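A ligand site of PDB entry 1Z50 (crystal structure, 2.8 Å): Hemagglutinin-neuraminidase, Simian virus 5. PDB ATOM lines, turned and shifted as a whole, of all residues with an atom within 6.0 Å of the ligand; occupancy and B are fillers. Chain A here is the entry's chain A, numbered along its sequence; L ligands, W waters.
Water W4 lies within hydrogen-bond range of an oxygen (O6) of the ligand (2.8 Å), the backbone NH (N) of Glu 357 (3.0 Å) and the guanidinium group (NE) of Arg 372 (3.3 Å). Water W1 lies within hydrogen-bond range of the side-chain carboxylate (OE2) of Glu 357 (2.8 Å), the side-chain hydroxyl (OG) of Ser 193 (2.8 Å), the side-chain hydroxyl (OH) of Tyr 273 (2.8 Å) and a nitrogen (N1) of the ligand (2.9 Å). Water W3 bridges the side-chain hydroxyl of Tyr 218 (2.9 Å) and an oxygen (O7) of the ligand (2.9 Å). Water W5 bridges the side-chain amide nitrogen (ND2) of Asn 374 (3.2 Å) and the backbone carbonyl oxygen (O) of Leu 426 (3.3 Å).
Ile 131 touches the ligand (CD1 to O3, 3.96 Å). CE2 of Phe 208 touches C11 of the ligand, 3.8 Å away. ND2 of Asn 255 touches C11 of the ligand (3.4 Å). Phe 320 touches the ligand. CG of Glu 357 touches O6 of the ligand (3.7 Å). Asn 374 touches the ligand (ND2 to C9, 3.7 Å). Hydrophobic or aromatic side chains within 4 Å of the ligand: Ile 131, Phe 208, Tyr 273, Phe 320 and Tyr 490. Of the 21 residues printed, 12 come within 4 Å of the ligand.
The side-chain carboxylate of Glu 214 sits at hydrogen-bond distance from an oxygen (O5) of the ligand (2.5 Å). The guanidinium group (NH2) of Arg 462 lies within salt-bridge range of an oxygen (O2) of the ligand, at 2.6 Å. An oxygen (O4) of the ligand sits close to the side-chain hydroxyl of Tyr 490 (3.3 Å). An oxygen (O1) of the ligand lies within salt-bridge range of the guanidinium group of Arg 130 (3.0 Å). The guanidinium group (NH2) of Arg 372 is in salt-bridge range of an oxygen (O2) of the ligand, 3.0 Å away. An oxygen (O6) of the ligand sits at hydrogen-bond distance from the side-chain hydroxyl (OH) of Tyr 273.
O of Gly 428 is in hydrogen-bond range of NH2 of Arg 462 (2.8 Å). The guanidinium group of Arg 372 is in hydrogen-bond range of the side-chain hydroxyl of Tyr 490 (2.8 Å). OE2 of Glu 357 sits at hydrogen-bond distance from OH of Tyr 490. OD1 of Asn 374 is in hydrogen-bond range of NH2 of Arg 372 (3.0 Å). The guanidinium group (NH2) of Arg 372 sits at hydrogen-bond distance from the backbone carbonyl oxygen (O) of Gly 428 (3.0 Å). The backbone NH (N) of Asn 255 sits at hydrogen-bond distance from the backbone carbonyl oxygen (O) of Tyr 273 (2.8 Å). The side-chain amide oxygen (OD1) of Asn 374 lies within hydrogen-bond range of the backbone NH (N) of Gly 428 (3.4 Å). N of Lys 192 is in hydrogen-bond range of O of Phe 208.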
ATOM      1  N   ARG A 130      -7.733  27.444   2.562  1.00  0.00           N
ATOM      2  CA  ARG A 130      -6.547  26.620   2.785  1.00  0.00           C
ATOM      3  C   ARG A 130      -5.251  27.334   2.470  1.00  0.00           C
ATOM      4  O   ARG A 130      -5.257  28.427   1.917  1.00  0.00           O
ATOM      5  CB  ARG A 130      -6.582  25.367   1.921  1.00  0.00           C
ATOM      6  CG  ARG A 130      -7.437  24.227   2.431  1.00  0.00           C
ATOM      7  CD  ARG A 130      -6.874  22.932   1.861  1.00  0.00           C
ATOM      8  NE  ARG A 130      -5.562  22.638   2.454  1.00  0.00           N
ATOM      9  CZ  ARG A 130      -4.711  21.750   1.976  1.00  0.00           C
ATOM     10  NH1 ARG A 130      -5.007  21.052   0.887  1.00  0.00           N
ATOM     11  NH2 ARG A 130      -3.552  21.544   2.597  1.00  0.00           N
ATOM     12  N   ILE A 131      -4.154  26.683   2.827  1.00  0.00           N
ATOM     13  CA  ILE A 131      -2.799  27.165   2.589  1.00  0.00           C
ATOM     14  C   ILE A 131      -2.488  28.524   3.213  1.00  0.00           C
ATOM     15  O   ILE A 131      -2.381  29.530   2.510  1.00  0.00           O
ATOM     16  CB  ILE A 131      -2.507  27.250   1.085  1.00  0.00           C
ATOM     17  CG1 ILE A 131      -2.997  25.967   0.401  1.00  0.00           C
ATOM     18  CG2 ILE A 131      -1.023  27.429   0.841  1.00  0.00           C
ATOM     19  CD1 ILE A 131      -2.468  24.693   1.042  1.00  0.00           C
ATOM     20  N   LYS A 192      -1.609  31.452  -6.193  1.00  0.00           N
ATOM     21  CA  LYS A 192      -1.567  30.238  -5.369  1.00  0.00           C
ATOM     22  C   LYS A 192      -0.253  30.002  -4.657  1.00  0.00           C
ATOM     23  O   LYS A 192       0.764  30.634  -4.969  1.00  0.00           O
ATOM     24  CB  LYS A 192      -1.848  29.019  -6.240  1.00  0.00           C
ATOM     25  CG  LYS A 192      -3.209  28.986  -6.900  1.00  0.00           C
ATOM     26  CD  LYS A 192      -4.285  28.596  -5.927  1.00  0.00           C
ATOM     27  CE  LYS A 192      -5.415  27.924  -6.680  1.00  0.00           C
ATOM     28  NZ  LYS A 192      -6.460  27.418  -5.747  1.00  0.00           N
ATOM     29  N   SER A 193      -0.283  29.074  -3.704  1.00  0.00           N
ATOM     30  CA  SER A 193       0.910  28.686  -2.953  1.00  0.00           C
ATOM     31  C   SER A 193       1.643  29.925  -2.432  1.00  0.00           C
ATOM     32  O   SER A 193       2.859  29.933  -2.321  1.00  0.00           O
ATOM     33  CB  SER A 193       1.804  27.862  -3.877  1.00  0.00           C
ATOM     34  OG  SER A 193       2.688  27.019  -3.167  1.00  0.00           O
ATOM     35  N   PHE A 208       2.373  32.476  -7.313  1.00  0.00           N
ATOM     36  CA  PHE A 208       2.561  32.106  -8.710  1.00  0.00           C
ATOM     37  C   PHE A 208       1.128  32.036  -9.219  1.00  0.00           C
ATOM     38  O   PHE A 208       0.212  31.793  -8.448  1.00  0.00           O
ATOM     39  CB  PHE A 208       3.297  30.756  -8.831  1.00  0.00           C
ATOM     40  CG  PHE A 208       2.400  29.534  -8.747  1.00  0.00           C
ATOM     41  CD1 PHE A 208       1.865  28.969  -9.905  1.00  0.00           C
ATOM     42  CD2 PHE A 208       2.163  28.909  -7.538  1.00  0.00           C
ATOM     43  CE1 PHE A 208       1.113  27.794  -9.838  1.00  0.00           C
ATOM     44  CE2 PHE A 208       1.415  27.734  -7.458  1.00  0.00           C
ATOM     45  CZ  PHE A 208       0.892  27.175  -8.613  1.00  0.00           C
ATOM     46  N   GLU A 214      -1.555  21.057 -11.174  1.00  0.00           N
ATOM     47  CA  GLU A 214      -0.159  21.061 -10.787  1.00  0.00           C
ATOM     48  C   GLU A 214       0.721  20.194 -11.669  1.00  0.00           C
ATOM     49  O   GLU A 214       1.777  20.618 -12.114  1.00  0.00           O
ATOM     50  CB  GLU A 214      -0.016  20.617  -9.338  1.00  0.00           C
ATOM     51  CG  GLU A 214       1.422  20.324  -8.929  1.00  0.00           C
ATOM     52  CD  GLU A 214       1.572  20.175  -7.445  1.00  0.00           C
ATOM     53  OE1 GLU A 214       0.784  19.399  -6.859  1.00  0.00           O
ATOM     54  OE2 GLU A 214       2.465  20.824  -6.859  1.00  0.00           O
ATOM     55  N   TYR A 218       4.480  20.742 -14.371  1.00  0.00           N
ATOM     56  CA  TYR A 218       5.770  20.080 -14.495  1.00  0.00           C
ATOM     57  C   TYR A 218       6.076  19.585 -15.901  1.00  0.00           C
ATOM     58  O   TYR A 218       7.241  19.481 -16.302  1.00  0.00           O
ATOM     59  CB  TYR A 218       5.855  18.925 -13.499  1.00  0.00           C
ATOM     60  CG  TYR A 218       5.991  19.383 -12.075  1.00  0.00           C
ATOM     61  CD1 TYR A 218       4.873  19.701 -11.309  1.00  0.00           C
ATOM     62  CD2 TYR A 218       7.247  19.567 -11.499  1.00  0.00           C
ATOM     63  CE1 TYR A 218       5.002  20.179 -10.010  1.00  0.00           C
ATOM     64  CE2 TYR A 218       7.392  20.049 -10.205  1.00  0.00           C
ATOM     65  CZ  TYR A 218       6.261  20.357  -9.465  1.00  0.00           C
ATOM     66  OH  TYR A 218       6.393  20.842  -8.189  1.00  0.00           O
ATOM     67  N   ASN A 255       7.322  27.415  -7.448  1.00  0.00           N
ATOM     68  CA  ASN A 255       6.292  27.820  -6.487  1.00  0.00           C
ATOM     69  C   ASN A 255       6.868  28.364  -5.201  1.00  0.00           C
ATOM     70  O   ASN A 255       8.000  28.049  -4.832  1.00  0.00           O
ATOM     71  CB  ASN A 255       5.424  26.633  -6.047  1.00  0.00           C
ATOM     72  CG  ASN A 255       4.702  25.964  -7.166  1.00  0.00           C
ATOM     73  OD1 ASN A 255       4.589  26.495  -8.274  1.00  0.00           O
ATOM     74  ND2 ASN A 255       4.164  24.784  -6.887  1.00  0.00           N
ATOM     75  N   TYR A 273      10.268  26.012  -4.435  1.00  0.00           N
ATOM     76  CA  TYR A 273      10.498  24.641  -4.880  1.00  0.00           C
ATOM     77  C   TYR A 273       9.862  24.491  -6.249  1.00  0.00           C
ATOM     78  O   TYR A 273       9.087  25.350  -6.675  1.00  0.00           O
ATOM     79  CB  TYR A 273       9.950  23.616  -3.868  1.00  0.00           C
ATOM     80  CG  TYR A 273       8.461  23.405  -3.890  1.00  0.00           C
ATOM     81  CD1 TYR A 273       7.580  24.364  -3.379  1.00  0.00           C
ATOM     82  CD2 TYR A 273       7.919  22.220  -4.399  1.00  0.00           C
ATOM     83  CE1 TYR A 273       6.203  24.144  -3.371  1.00  0.00           C
ATOM     84  CE2 TYR A 273       6.545  21.997  -4.400  1.00  0.00           C
ATOM     85  CZ  TYR A 273       5.689  22.958  -3.890  1.00  0.00           C
ATOM     86  OH  TYR A 273       4.333  22.720  -3.866  1.00  0.00           O
ATOM     87  N   PHE A 320       5.940  13.670 -12.247  1.00  0.00           N
ATOM     88  CA  PHE A 320       5.912  15.117 -12.420  1.00  0.00           C
ATOM     89  C   PHE A 320       6.806  15.545 -13.578  1.00  0.00           C
ATOM     90  O   PHE A 320       7.823  16.212 -13.377  1.00  0.00           O
ATOM     91  CB  PHE A 320       6.322  15.836 -11.138  1.00  0.00           C
ATOM     92  CG  PHE A 320       5.176  16.132 -10.207  1.00  0.00           C
ATOM     93  CD1 PHE A 320       3.863  15.971 -10.622  1.00  0.00           C
ATOM     94  CD2 PHE A 320       5.419  16.605  -8.923  1.00  0.00           C
ATOM     95  CE1 PHE A 320       2.797  16.268  -9.769  1.00  0.00           C
ATOM     96  CE2 PHE A 320       4.362  16.899  -8.065  1.00  0.00           C
ATOM     97  CZ  PHE A 320       3.052  16.736  -8.489  1.00  0.00           C
ATOM     98  N   ALA A 356      10.392  20.616  -1.901  1.00  0.00           N
ATOM     99  CA  ALA A 356       9.069  20.597  -1.269  1.00  0.00           C
ATOM    100  C   ALA A 356       8.723  21.975  -0.718  1.00  0.00           C
ATOM    101  O   ALA A 356       9.536  22.908  -0.783  1.00  0.00           O
ATOM    102  CB  ALA A 356       9.039  19.572  -0.138  1.00  0.00           C
ATOM    103  N   GLU A 357       7.515  22.103  -0.184  1.00  0.00           N
ATOM    104  CA  GLU A 357       7.093  23.366   0.414  1.00  0.00           C
ATOM    105  C   GLU A 357       8.036  23.558   1.577  1.00  0.00           C
ATOM    106  O   GLU A 357       8.657  22.607   2.054  1.00  0.00           O
ATOM    107  CB  GLU A 357       5.651  23.272   0.935  1.00  0.00           C
ATOM    108  CG  GLU A 357       4.613  22.915  -0.115  1.00  0.00           C
ATOM    109  CD  GLU A 357       3.253  22.659   0.505  1.00  0.00           C
ATOM    110  OE1 GLU A 357       3.190  21.913   1.500  1.00  0.00           O
ATOM    111  OE2 GLU A 357       2.249  23.197  -0.003  1.00  0.00           O
ATOM    112  N   ARG A 372       9.372  20.569   4.000  1.00  0.00           N
ATOM    113  CA  ARG A 372       8.333  19.569   4.088  1.00  0.00           C
ATOM    114  C   ARG A 372       8.938  18.243   3.660  1.00  0.00           C
ATOM    115  O   ARG A 372       9.741  18.183   2.716  1.00  0.00           O
ATOM    116  CB  ARG A 372       7.165  19.947   3.180  1.00  0.00           C
ATOM    117  CG  ARG A 372       6.125  18.851   2.954  1.00  0.00           C
ATOM    118  CD  ARG A 372       4.926  19.381   2.191  1.00  0.00           C
ATOM    119  NE  ARG A 372       4.181  18.315   1.540  1.00  0.00           N
ATOM    120  CZ  ARG A 372       2.939  18.435   1.080  1.00  0.00           C
ATOM    121  NH1 ARG A 372       2.291  19.586   1.201  1.00  0.00           N
ATOM    122  NH2 ARG A 372       2.344  17.413   0.484  1.00  0.00           N
ATOM    123  N   ASN A 374       8.284  15.535   1.812  1.00  0.00           N
ATOM    124  CA  ASN A 374       7.420  15.020   0.763  1.00  0.00           C
ATOM    125  C   ASN A 374       8.143  13.862   0.073  1.00  0.00           C
ATOM    126  O   ASN A 374       7.672  13.345  -0.934  1.00  0.00           O
ATOM    127  CB  ASN A 374       7.111  16.123  -0.248  1.00  0.00           C
ATOM    128  CG  ASN A 374       5.739  15.993  -0.860  1.00  0.00           C
ATOM    129  OD1 ASN A 374       4.746  15.805  -0.152  1.00  0.00           O
ATOM    130  ND2 ASN A 374       5.659  16.102  -2.174  1.00  0.00           N
ATOM    131  N   LEU A 426       6.597  10.754  -3.112  1.00  0.00           N
ATOM    132  CA  LEU A 426       6.018  12.044  -3.460  1.00  0.00           C
ATOM    133  C   LEU A 426       4.698  12.138  -2.702  1.00  0.00           C
ATOM    134  O   LEU A 426       3.618  12.219  -3.283  1.00  0.00           O
ATOM    135  CB  LEU A 426       5.778  12.138  -4.967  1.00  0.00           C
ATOM    136  CG  LEU A 426       5.314  13.480  -5.553  1.00  0.00           C
ATOM    137  CD1 LEU A 426       6.344  14.554  -5.280  1.00  0.00           C
ATOM    138  CD2 LEU A 426       5.091  13.331  -7.044  1.00  0.00           C
ATOM    139  N   GLY A 428       3.078  13.370   1.554  1.00  0.00           N
ATOM    140  CA  GLY A 428       3.385  13.999   2.818  1.00  0.00           C
ATOM    141  C   GLY A 428       2.481  15.175   3.158  1.00  0.00           C
ATOM    142  O   GLY A 428       1.440  15.376   2.535  1.00  0.00           O
ATOM    143  N   VAL A 429       2.874  15.952   4.162  1.00  0.00           N
ATOM    144  CA  VAL A 429       2.111  17.125   4.590  1.00  0.00           C
ATOM    145  C   VAL A 429       3.053  18.187   5.078  1.00  0.00           C
ATOM    146  O   VAL A 429       4.192  17.893   5.468  1.00  0.00           O
ATOM    147  CB  VAL A 429       1.175  16.860   5.793  1.00  0.00           C
ATOM    148  CG1 VAL A 429      -0.255  17.141   5.402  1.00  0.00           C
ATOM    149  CG2 VAL A 429       1.362  15.462   6.329  1.00  0.00           C
ATOM    150  N   TYR A 430       2.574  19.414   5.069  1.00  0.00           N
ATOM    151  CA  TYR A 430       3.351  20.522   5.560  1.00  0.00           C
ATOM    152  C   TYR A 430       3.087  20.589   7.063  1.00  0.00           C
ATOM    153  O   TYR A 430       1.923  20.653   7.501  1.00  0.00           O
ATOM    154  CB  TYR A 430       2.914  21.829   4.883  1.00  0.00           C
ATOM    155  CG  TYR A 430       3.603  23.057   5.433  1.00  0.00           C
ATOM    156  CD1 TYR A 430       3.281  23.551   6.696  1.00  0.00           C
ATOM    157  CD2 TYR A 430       4.604  23.707   4.709  1.00  0.00           C
ATOM    158  CE1 TYR A 430       3.933  24.639   7.228  1.00  0.00           C
ATOM    159  CE2 TYR A 430       5.264  24.801   5.232  1.00  0.00           C
ATOM    160  CZ  TYR A 430       4.931  25.267   6.498  1.00  0.00           C
ATOM    161  OH  TYR A 430       5.601  26.328   7.047  1.00  0.00           O
ATOM    162  N   ARG A 462      -4.541  11.912   7.028  1.00  0.00           N
ATOM    163  CA  ARG A 462      -4.351  13.254   7.557  1.00  0.00           C
ATOM    164  C   ARG A 462      -5.363  13.380   8.682  1.00  0.00           C
ATOM    165  O   ARG A 462      -6.374  14.072   8.579  1.00  0.00           O
ATOM    166  CB  ARG A 462      -4.582  14.293   6.475  1.00  0.00           C
ATOM    167  CG  ARG A 462      -3.513  14.228   5.414  1.00  0.00           C
ATOM    168  CD  ARG A 462      -3.576  15.419   4.507  1.00  0.00           C
ATOM    169  NE  ARG A 462      -2.400  15.490   3.656  1.00  0.00           N
ATOM    170  CZ  ARG A 462      -2.177  16.472   2.796  1.00  0.00           C
ATOM    171  NH1 ARG A 462      -3.059  17.458   2.682  1.00  0.00           N
ATOM    172  NH2 ARG A 462      -1.073  16.479   2.059  1.00  0.00           N
ATOM    173  N   ALA A 489      -4.992  19.264   8.168  1.00  0.00           N
ATOM    174  CA  ALA A 489      -4.017  19.299   7.079  1.00  0.00           C
ATOM    175  C   ALA A 489      -2.706  19.945   7.533  1.00  0.00           C
ATOM    176  O   ALA A 489      -1.996  19.384   8.362  1.00  0.00           O
ATOM    177  CB  ALA A 489      -4.600  20.021   5.881  1.00  0.00           C
ATOM    178  N   TYR A 490      -2.392  21.116   6.986  1.00  0.00           N
ATOM    179  CA  TYR A 490      -1.156  21.821   7.332  1.00  0.00           C
ATOM    180  C   TYR A 490      -1.167  22.402   8.730  1.00  0.00           C
ATOM    181  O   TYR A 490      -2.223  22.588   9.348  1.00  0.00           O
ATOM    182  CB  TYR A 490      -0.889  22.966   6.361  1.00  0.00           C
ATOM    183  CG  TYR A 490      -0.590  22.570   4.942  1.00  0.00           C
ATOM    184  CD1 TYR A 490      -0.701  21.242   4.513  1.00  0.00           C
ATOM    185  CD2 TYR A 490      -0.189  23.526   4.023  1.00  0.00           C
ATOM    186  CE1 TYR A 490      -0.405  20.893   3.192  1.00  0.00           C
ATOM    187  CE2 TYR A 490       0.107  23.189   2.710  1.00  0.00           C
ATOM    188  CZ  TYR A 490      -0.003  21.875   2.310  1.00  0.00           C
ATOM    189  OH  TYR A 490       0.328  21.569   1.015  1.00  0.00           O
HETATM  190  C1  LIG L   1      -1.349  19.282  -0.068  1.00  0.00           C
HETATM  191  C2  LIG L   1      -1.007  20.201  -1.117  1.00  0.00           C
HETATM  192  C3  LIG L   1      -1.826  21.459  -1.289  1.00  0.00           C
HETATM  193  C4  LIG L   1      -1.074  22.509  -2.138  1.00  0.00           C
HETATM  194  C5  LIG L   1      -0.272  21.863  -3.239  1.00  0.00           C
HETATM  195  C6  LIG L   1       0.745  20.903  -2.581  1.00  0.00           C
HETATM  196  C7  LIG L   1       1.617  20.162  -3.609  1.00  0.00           C
HETATM  197  C8  LIG L   1       2.669  19.273  -2.969  1.00  0.00           C
HETATM  198  C9  LIG L   1       3.525  18.504  -4.007  1.00  0.00           C
HETATM  199  C10 LIG L   1       0.231  23.172  -5.286  1.00  0.00           C
HETATM  200  C11 LIG L   1       0.972  24.319  -5.930  1.00  0.00           C
HETATM  201  N1  LIG L   1       0.375  22.947  -3.986  1.00  0.00           N
HETATM  202  O1  LIG L   1      -2.555  19.339   0.592  1.00  0.00           O
HETATM  203  O2  LIG L   1      -0.500  18.375   0.304  1.00  0.00           O
HETATM  204  O3  LIG L   1      -2.046  23.411  -2.677  1.00  0.00           O
HETATM  205  O4  LIG L   1       0.018  19.883  -1.844  1.00  0.00           O
HETATM  206  O5  LIG L   1       0.812  19.299  -4.395  1.00  0.00           O
HETATM  207  O6  LIG L   1       3.541  20.099  -2.175  1.00  0.00           O
HETATM  208  O7  LIG L   1       4.126  19.328  -4.978  1.00  0.00           O
HETATM  209  O8  LIG L   1      -0.570  22.403  -6.088  1.00  0.00           O
HETATM  210  O   HOH W   1       2.468  24.332  -2.522  1.00  0.00           O
HETATM  211  O   HOH W   2      -1.831  25.835  -4.669  1.00  0.00           O
HETATM  212  O   HOH W   3       6.762  18.861  -6.142  1.00  0.00           O
HETATM  213  O   HOH W   4       5.974  19.618  -0.859  1.00  0.00           O
HETATM  214  O   HOH W   5       2.608  15.340  -2.954  1.00  0.00           O
